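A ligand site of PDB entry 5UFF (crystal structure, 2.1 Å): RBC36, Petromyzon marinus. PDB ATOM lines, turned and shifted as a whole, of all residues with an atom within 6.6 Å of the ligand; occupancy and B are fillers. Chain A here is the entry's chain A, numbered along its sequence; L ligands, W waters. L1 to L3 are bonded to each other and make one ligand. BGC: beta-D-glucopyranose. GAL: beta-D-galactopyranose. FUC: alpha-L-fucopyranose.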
ATOM      1  N   ARG A  15      31.748 -17.393 -21.908  1.00  0.00           N
ATOM      2  CA  ARG A  15      31.351 -16.057 -22.353  1.00  0.00           C
ATOM      3  C   ARG A  15      32.229 -15.601 -23.513  1.00  0.00           C
ATOM      4  O   ARG A  15      33.410 -15.917 -23.560  1.00  0.00           O
ATOM      5  CB  ARG A  15      31.436 -15.026 -21.223  1.00  0.00           C
ATOM      6  CG  ARG A  15      32.821 -14.708 -20.778  1.00  0.00           C
ATOM      7  CD  ARG A  15      32.818 -13.965 -19.484  1.00  0.00           C
ATOM      8  NE  ARG A  15      33.330 -14.763 -18.390  1.00  0.00           N
ATOM      9  CZ  ARG A  15      33.344 -14.375 -17.124  1.00  0.00           C
ATOM     10  NH1 ARG A  15      33.833 -15.176 -16.186  1.00  0.00           N
ATOM     11  NH2 ARG A  15      32.873 -13.176 -16.795  1.00  0.00           N
ATOM     12  N   HIS A  36      26.892 -15.829 -21.271  1.00  0.00           N
ATOM     13  CA  HIS A  36      26.527 -14.510 -21.736  1.00  0.00           C
ATOM     14  C   HIS A  36      27.542 -13.985 -22.779  1.00  0.00           C
ATOM     15  O   HIS A  36      28.721 -14.309 -22.720  1.00  0.00           O
ATOM     16  CB  HIS A  36      26.406 -13.555 -20.547  1.00  0.00           C
ATOM     17  CG  HIS A  36      27.707 -13.279 -19.848  1.00  0.00           C
ATOM     18  ND1 HIS A  36      28.274 -14.153 -18.962  1.00  0.00           N
ATOM     19  CD2 HIS A  36      28.532 -12.203 -19.895  1.00  0.00           C
ATOM     20  CE1 HIS A  36      29.412 -13.645 -18.498  1.00  0.00           C
ATOM     21  NE2 HIS A  36      29.586 -12.460 -19.050  1.00  0.00           N
ATOM     22  N   TYR A  58      24.272 -17.489 -16.462  1.00  0.00           N
ATOM     23  CA  TYR A  58      24.230 -16.234 -17.173  1.00  0.00           C
ATOM     24  C   TYR A  58      23.999 -16.420 -18.669  1.00  0.00           C
ATOM     25  O   TYR A  58      24.774 -17.063 -19.370  1.00  0.00           O
ATOM     26  CB  TYR A  58      25.518 -15.448 -16.928  1.00  0.00           C
ATOM     27  CG  TYR A  58      25.796 -15.186 -15.455  1.00  0.00           C
ATOM     28  CD1 TYR A  58      25.377 -14.006 -14.839  1.00  0.00           C
ATOM     29  CD2 TYR A  58      26.488 -16.125 -14.695  1.00  0.00           C
ATOM     30  CE1 TYR A  58      25.650 -13.755 -13.500  1.00  0.00           C
ATOM     31  CE2 TYR A  58      26.763 -15.886 -13.362  1.00  0.00           C
ATOM     32  CZ  TYR A  58      26.350 -14.699 -12.775  1.00  0.00           C
ATOM     33  OH  TYR A  58      26.633 -14.476 -11.442  1.00  0.00           O
ATOM     34  N   GLY A  60      22.781 -13.616 -20.496  1.00  0.00           N
ATOM     35  CA  GLY A  60      22.698 -12.258 -21.001  1.00  0.00           C
ATOM     36  C   GLY A  60      23.370 -12.084 -22.356  1.00  0.00           C
ATOM     37  O   GLY A  60      24.217 -12.878 -22.743  1.00  0.00           O
ATOM     38  N   SER A  61      22.939 -11.061 -23.095  1.00  0.00           N
ATOM     39  CA  SER A  61      23.579 -10.668 -24.353  1.00  0.00           C
ATOM     40  C   SER A  61      23.658 -11.799 -25.359  1.00  0.00           C
ATOM     41  O   SER A  61      24.744 -12.134 -25.834  1.00  0.00           O
ATOM     42  CB  SER A  61      24.973 -10.112 -24.080  1.00  0.00           C
ATOM     43  OG  SER A  61      24.903  -8.956 -23.287  1.00  0.00           O
ATOM     44  N   ASP A  82      20.553 -14.600 -15.211  1.00  0.00           N
ATOM     45  CA  ASP A  82      20.732 -13.389 -16.025  1.00  0.00           C
ATOM     46  C   ASP A  82      20.277 -13.575 -17.473  1.00  0.00           C
ATOM     47  O   ASP A  82      20.875 -14.343 -18.226  1.00  0.00           O
ATOM     48  CB  ASP A  82      22.192 -12.939 -16.007  1.00  0.00           C
ATOM     49  CG  ASP A  82      22.377 -11.501 -16.498  1.00  0.00           C
ATOM     50  OD1 ASP A  82      21.591 -11.020 -17.356  1.00  0.00           O
ATOM     51  OD2 ASP A  82      23.344 -10.842 -16.026  1.00  0.00           O
ATOM     52  N   GLY A  84      19.310 -10.606 -19.375  1.00  0.00           N
ATOM     53  CA  GLY A  84      19.311  -9.280 -19.946  1.00  0.00           C
ATOM     54  C   GLY A  84      19.871  -9.275 -21.355  1.00  0.00           C
ATOM     55  O   GLY A  84      20.765 -10.046 -21.664  1.00  0.00           O
ATOM     56  N   THR A  85      19.309  -8.435 -22.205  1.00  0.00           N
ATOM     57  CA  THR A  85      19.859  -8.167 -23.533  1.00  0.00           C
ATOM     58  C   THR A  85      19.642  -9.373 -24.420  1.00  0.00           C
ATOM     59  O   THR A  85      20.567  -9.953 -24.990  1.00  0.00           O
ATOM     60  CB  THR A  85      21.364  -7.748 -23.469  1.00  0.00           C
ATOM     61  OG1 THR A  85      21.524  -6.670 -22.544  1.00  0.00           O
ATOM     62  CG2 THR A  85      21.875  -7.294 -24.842  1.00  0.00           C
ATOM     63  N   PHE A 106      17.959 -10.895 -13.517  1.00  0.00           N
ATOM     64  CA  PHE A 106      18.246  -9.830 -14.434  1.00  0.00           C
ATOM     65  C   PHE A 106      17.555 -10.064 -15.762  1.00  0.00           C
ATOM     66  O   PHE A 106      17.801 -11.069 -16.413  1.00  0.00           O
ATOM     67  CB  PHE A 106      19.754  -9.708 -14.621  1.00  0.00           C
ATOM     68  CG  PHE A 106      20.496  -9.567 -13.329  1.00  0.00           C
ATOM     69  CD1 PHE A 106      20.442  -8.387 -12.608  1.00  0.00           C
ATOM     70  CD2 PHE A 106      21.200 -10.640 -12.805  1.00  0.00           C
ATOM     71  CE1 PHE A 106      21.106  -8.254 -11.390  1.00  0.00           C
ATOM     72  CE2 PHE A 106      21.870 -10.510 -11.594  1.00  0.00           C
ATOM     73  CZ  PHE A 106      21.826  -9.313 -10.887  1.00  0.00           C
ATOM     74  N   MET A 107      16.701  -9.138 -16.167  1.00  0.00           N
ATOM     75  CA  MET A 107      15.934  -9.287 -17.388  1.00  0.00           C
ATOM     76  C   MET A 107      15.888  -8.022 -18.213  1.00  0.00           C
ATOM     77  O   MET A 107      15.029  -7.884 -19.074  1.00  0.00           O
ATOM     78  CB  MET A 107      14.508  -9.692 -17.066  1.00  0.00           C
ATOM     79  CG  MET A 107      14.401 -10.972 -16.296  1.00  0.00           C
ATOM     80  SD  MET A 107      12.726 -11.533 -16.544  1.00  0.00           S
ATOM     81  CE  MET A 107      12.895 -12.100 -18.242  1.00  0.00           C
ATOM     82  N   CYS A 108      16.817  -7.114 -17.952  1.00  0.00           N
ATOM     83  CA  CYS A 108      16.841  -5.835 -18.641  1.00  0.00           C
ATOM     84  C   CYS A 108      16.922  -5.997 -20.154  1.00  0.00           C
ATOM     85  O   CYS A 108      17.261  -7.068 -20.649  1.00  0.00           O
ATOM     86  CB  CYS A 108      18.027  -5.006 -18.189  1.00  0.00           C
ATOM     87  SG  CYS A 108      19.369  -5.059 -19.423  1.00  0.00           S
ATOM     88  N   CYS A 109      16.611  -4.922 -20.876  1.00  0.00           N
ATOM     89  CA  CYS A 109      16.997  -4.786 -22.268  1.00  0.00           C
ATOM     90  C   CYS A 109      16.506  -5.967 -23.125  1.00  0.00           C
ATOM     91  O   CYS A 109      17.228  -6.465 -23.996  1.00  0.00           O
ATOM     92  CB  CYS A 109      18.527  -4.629 -22.391  1.00  0.00           C
ATOM     93  SG  CYS A 109      19.320  -3.730 -21.002  1.00  0.00           S
ATOM     94  N   HIS A 127      17.846  -8.882  -5.976  1.00  0.00           N
ATOM     95  CA  HIS A 127      17.939  -8.016  -7.134  1.00  0.00           C
ATOM     96  C   HIS A 127      16.885  -8.387  -8.152  1.00  0.00           C
ATOM     97  O   HIS A 127      16.684  -9.555  -8.459  1.00  0.00           O
ATOM     98  CB  HIS A 127      19.326  -8.068  -7.799  1.00  0.00           C
ATOM     99  CG  HIS A 127      20.467  -7.741  -6.882  1.00  0.00           C
ATOM    100  ND1 HIS A 127      20.651  -8.341  -5.661  1.00  0.00           N
ATOM    101  CD2 HIS A 127      21.498  -6.882  -7.033  1.00  0.00           C
ATOM    102  CE1 HIS A 127      21.741  -7.853  -5.085  1.00  0.00           C
ATOM    103  NE2 HIS A 127      22.277  -6.975  -5.900  1.00  0.00           N
ATOM    104  N   ALA A 129      15.873  -6.811 -12.052  1.00  0.00           N
ATOM    105  CA  ALA A 129      16.160  -5.826 -13.094  1.00  0.00           C
ATOM    106  C   ALA A 129      15.187  -5.907 -14.269  1.00  0.00           C
ATOM    107  O   ALA A 129      15.192  -6.884 -15.008  1.00  0.00           O
ATOM    108  CB  ALA A 129      17.576  -5.990 -13.584  1.00  0.00           C
ATOM    109  N   LEU A 130      14.384  -4.867 -14.443  1.00  0.00           N
ATOM    110  CA  LEU A 130      13.399  -4.817 -15.518  1.00  0.00           C
ATOM    111  C   LEU A 130      13.630  -3.680 -16.497  1.00  0.00           C
ATOM    112  O   LEU A 130      12.819  -3.432 -17.382  1.00  0.00           O
ATOM    113  CB  LEU A 130      12.002  -4.683 -14.934  1.00  0.00           C
ATOM    114  CG  LEU A 130      11.628  -5.771 -13.941  1.00  0.00           C
ATOM    115  CD1 LEU A 130      10.315  -5.454 -13.262  1.00  0.00           C
ATOM    116  CD2 LEU A 130      11.552  -7.088 -14.690  1.00  0.00           C
ATOM    117  N   ASP A 131      14.747  -2.979 -16.333  1.00  0.00           N
ATOM    118  CA  ASP A 131      14.985  -1.751 -17.054  1.00  0.00           C
ATOM    119  C   ASP A 131      15.114  -1.958 -18.556  1.00  0.00           C
ATOM    120  O   ASP A 131      15.570  -2.996 -19.012  1.00  0.00           O
ATOM    121  CB  ASP A 131      16.239  -1.075 -16.501  1.00  0.00           C
ATOM    122  CG  ASP A 131      17.449  -1.975 -16.551  1.00  0.00           C
ATOM    123  OD1 ASP A 131      17.505  -2.933 -15.737  1.00  0.00           O
ATOM    124  OD2 ASP A 131      18.340  -1.741 -17.389  1.00  0.00           O
ATOM    125  N   GLN A 132      14.683  -0.936 -19.309  1.00  0.00           N
ATOM    126  CA  GLN A 132      14.804  -0.916 -20.771  1.00  0.00           C
ATOM    127  C   GLN A 132      14.049  -2.052 -21.462  1.00  0.00           C
ATOM    128  O   GLN A 132      14.583  -2.725 -22.341  1.00  0.00           O
ATOM    129  CB  GLN A 132      16.271  -0.935 -21.180  1.00  0.00           C
ATOM    130  CG  GLN A 132      17.121   0.078 -20.437  1.00  0.00           C
ATOM    131  CD  GLN A 132      18.497   0.223 -21.019  1.00  0.00           C
ATOM    132  OE1 GLN A 132      18.661   0.743 -22.124  1.00  0.00           O
ATOM    133  NE2 GLN A 132      19.500  -0.234 -20.288  1.00  0.00           N
ATOM    134  N   TYR A 153      15.463  -2.349 -10.544  1.00  0.00           N
ATOM    135  CA  TYR A 153      15.767  -1.554 -11.726  1.00  0.00           C
ATOM    136  C   TYR A 153      14.535  -1.388 -12.596  1.00  0.00           C
ATOM    137  O   TYR A 153      14.089  -2.353 -13.219  1.00  0.00           O
ATOM    138  CB  TYR A 153      16.873  -2.196 -12.549  1.00  0.00           C
ATOM    139  CG  TYR A 153      18.165  -2.305 -11.813  1.00  0.00           C
ATOM    140  CD1 TYR A 153      18.386  -3.332 -10.906  1.00  0.00           C
ATOM    141  CD2 TYR A 153      19.172  -1.355 -11.990  1.00  0.00           C
ATOM    142  CE1 TYR A 153      19.557  -3.438 -10.232  1.00  0.00           C
ATOM    143  CE2 TYR A 153      20.359  -1.459 -11.315  1.00  0.00           C
ATOM    144  CZ  TYR A 153      20.548  -2.492 -10.437  1.00  0.00           C
ATOM    145  OH  TYR A 153      21.722  -2.622  -9.748  1.00  0.00           O
ATOM    146  N   PHE A 155      14.088   1.766 -14.662  1.00  0.00           N
ATOM    147  CA  PHE A 155      14.247   2.872 -15.607  1.00  0.00           C
ATOM    148  C   PHE A 155      14.150   2.420 -17.059  1.00  0.00           C
ATOM    149  O   PHE A 155      14.245   1.230 -17.361  1.00  0.00           O
ATOM    150  CB  PHE A 155      15.585   3.600 -15.358  1.00  0.00           C
ATOM    151  CG  PHE A 155      16.796   2.773 -15.637  1.00  0.00           C
ATOM    152  CD1 PHE A 155      17.459   2.111 -14.614  1.00  0.00           C
ATOM    153  CD2 PHE A 155      17.277   2.631 -16.930  1.00  0.00           C
ATOM    154  CE1 PHE A 155      18.573   1.343 -14.872  1.00  0.00           C
ATOM    155  CE2 PHE A 155      18.393   1.851 -17.194  1.00  0.00           C
ATOM    156  CZ  PHE A 155      19.038   1.220 -16.158  1.00  0.00           C
ATOM    157  N   TRP A 183      21.305   2.749 -13.348  1.00  0.00           N
ATOM    158  CA  TRP A 183      22.614   2.163 -13.655  1.00  0.00           C
ATOM    159  C   TRP A 183      23.609   3.165 -14.259  1.00  0.00           C
ATOM    160  O   TRP A 183      23.517   3.508 -15.438  1.00  0.00           O
ATOM    161  CB  TRP A 183      22.422   0.954 -14.605  1.00  0.00           C
ATOM    162  CG  TRP A 183      23.665   0.135 -14.813  1.00  0.00           C
ATOM    163  CD1 TRP A 183      24.499   0.158 -15.900  1.00  0.00           C
ATOM    164  CD2 TRP A 183      24.223  -0.834 -13.901  1.00  0.00           C
ATOM    165  NE1 TRP A 183      25.525  -0.735 -15.731  1.00  0.00           N
ATOM    166  CE2 TRP A 183      25.385  -1.354 -14.521  1.00  0.00           C
ATOM    167  CE3 TRP A 183      23.844  -1.323 -12.649  1.00  0.00           C
ATOM    168  CZ2 TRP A 183      26.181  -2.325 -13.912  1.00  0.00           C
ATOM    169  CZ3 TRP A 183      24.645  -2.285 -12.040  1.00  0.00           C
ATOM    170  CH2 TRP A 183      25.803  -2.782 -12.675  1.00  0.00           C
ATOM    171  N   GLY A 185      26.987   2.708 -14.992  1.00  0.00           N
ATOM    172  CA  GLY A 185      28.078   1.745 -15.023  1.00  0.00           C
ATOM    173  C   GLY A 185      28.147   0.867 -13.774  1.00  0.00           C
ATOM    174  O   GLY A 185      28.950  -0.074 -13.696  1.00  0.00           O
HETATM  175  C2  BGC L   1      26.276  -8.511 -16.693  1.00  0.00           C
HETATM  176  C3  BGC L   1      25.050  -7.740 -16.773  1.00  0.00           C
HETATM  177  C4  BGC L   1      25.302  -6.287 -16.532  1.00  0.00           C
HETATM  178  C5  BGC L   1      26.450  -5.757 -17.387  1.00  0.00           C
HETATM  179  C6  BGC L   1      26.946  -4.529 -16.879  1.00  0.00           C
HETATM  180  C1  BGC L   1      27.164  -8.102 -17.744  1.00  0.00           C
HETATM  181  O1  BGC L   1      28.291  -8.961 -17.792  1.00  0.00           O
HETATM  182  O2  BGC L   1      26.016  -9.970 -16.835  1.00  0.00           O
HETATM  183  O3  BGC L   1      24.063  -8.247 -15.786  1.00  0.00           O
HETATM  184  O4  BGC L   1      24.107  -5.629 -17.003  1.00  0.00           O
HETATM  185  O5  BGC L   1      27.613  -6.733 -17.414  1.00  0.00           O
HETATM  186  O6  BGC L   1      27.186  -3.679 -17.988  1.00  0.00           O
HETATM  187  C1  GAL L   2      23.659  -4.608 -16.156  1.00  0.00           C
HETATM  188  C2  GAL L   2      22.644  -3.845 -16.921  1.00  0.00           C
HETATM  189  C3  GAL L   2      21.990  -2.847 -16.116  1.00  0.00           C
HETATM  190  C4  GAL L   2      21.385  -3.414 -14.885  1.00  0.00           C
HETATM  191  C5  GAL L   2      22.366  -4.237 -14.048  1.00  0.00           C
HETATM  192  C6  GAL L   2      21.704  -4.948 -13.039  1.00  0.00           C
HETATM  193  O2  GAL L   2      23.342  -3.120 -18.007  1.00  0.00           O
HETATM  194  O3  GAL L   2      20.984  -2.133 -16.908  1.00  0.00           O
HETATM  195  O4  GAL L   2      20.181  -4.131 -15.172  1.00  0.00           O
HETATM  196  O5  GAL L   2      23.061  -5.247 -14.970  1.00  0.00           O
HETATM  197  O6  GAL L   2      22.696  -5.749 -12.471  1.00  0.00           O
HETATM  198  C1  FUC L   3      22.615  -3.121 -19.190  1.00  0.00           C
HETATM  199  C2  FUC L   3      22.866  -1.809 -19.864  1.00  0.00           C
HETATM  200  C3  FUC L   3      24.320  -1.619 -20.169  1.00  0.00           C
HETATM  201  C4  FUC L   3      24.909  -2.773 -20.913  1.00  0.00           C
HETATM  202  C5  FUC L   3      24.579  -4.126 -20.325  1.00  0.00           C
HETATM  203  C6  FUC L   3      24.925  -5.220 -21.265  1.00  0.00           C
HETATM  204  O2  FUC L   3      22.415  -0.731 -19.005  1.00  0.00           O
HETATM  205  O3  FUC L   3      24.517  -0.383 -20.934  1.00  0.00           O
HETATM  206  O4  FUC L   3      24.425  -2.686 -22.274  1.00  0.00           O
HETATM  207  O5  FUC L   3      23.165  -4.289 -19.935  1.00  0.00           O
HETATM  208  O   HOH W   1      19.766  -6.666 -16.041  1.00  0.00           O
HETATM  209  O   HOH W   2      24.516 -12.406 -18.289  1.00  0.00           O
HETATM  210  O   HOH W   3      21.817  -7.781 -17.168  1.00  0.00           O
HETATM  211  O   HOH W   4      27.390  -0.125 -20.796  1.00  0.00           O
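His 36 touches the ligand. Thr 85 touches the ligand. Phe 106 touches the ligand. SG of Cys 108 touches C1 of FUC L3 (3.8 Å). SG of Cys 109 touches C1 of FUC L3 (3.8 Å). Ala 129 touches the ligand. Tyr 153 touches the ligand. CZ of Phe 155 touches O3 of GAL L2 (3.9 Å). Trp 183 touches the ligand. Hydrophobic or aromatic side chains within 4 Å of the ligand: His 36, Phe 106, Ala 129, Tyr 153, Phe 155 and Trp 183. Of the 21 residues printed, 12 come within 4 Å of the ligand. Along chain A the residues within 4 Å of the ligand span positions 36 to 183. The nearest printed residue that does not touch the ligand is Ser 61 (4.2 Å).
The backbone NH (N) of Ser 61 lies close to the backbone carbonyl oxygen (O) of Thr 85. O of Ala 129 lies within hydrogen-bond range of N of Met 107 (2.9 Å). The backbone carbonyl oxygen (O) of Tyr 58 sits at hydrogen-bond distance from the backbone NH (N) of His 36, at 3.1 Å. The side-chain amide nitrogen (NE2) of Gln 132 is in hydrogen-bond range of the side-chain carboxylate (OD2) of Asp 131 (3.5 Å). The backbone NH (N) of Cys 108 is in hydrogen-bond range of the backbone carbonyl oxygen (O) of Ala 129 (3.4 Å). The backbone carbonyl oxygen (O) of Tyr 153 lies within hydrogen-bond range of the backbone NH (N) of Leu 130. The backbone carbonyl oxygen (O) of Gln 132 sits close to the backbone NH (N) of Cys 109 (3.3 Å). N of Cys 109 is in hydrogen-bond range of O of Asp 131 (2.9 Å).
O2 of FUC L3 is in hydrogen-bond range of NE2 of Gln 132. The side-chain carboxylate (OD2) of Asp 82 sits at hydrogen-bond distance from an oxygen (O3) of BGC L1 (2.7 Å). OD2 of Asp 131 lies within hydrogen-bond range of O3 of GAL L2 (2.7 Å).
Water W3 bridges O3 of BGC L1 (2.7 Å) and OD1 of Asp 82 (3.3 Å). Water W1 bridges O4 of GAL L2 and SG of Cys 108. Water W2 lies within hydrogen-bond range of the side-chain carboxylate (OD2) of Asp 82 (3.0 Å), the backbone NH (N) of Gly 60 (3.1 Å) and an oxygen (O2) of BGC L1 (3.2 Å).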
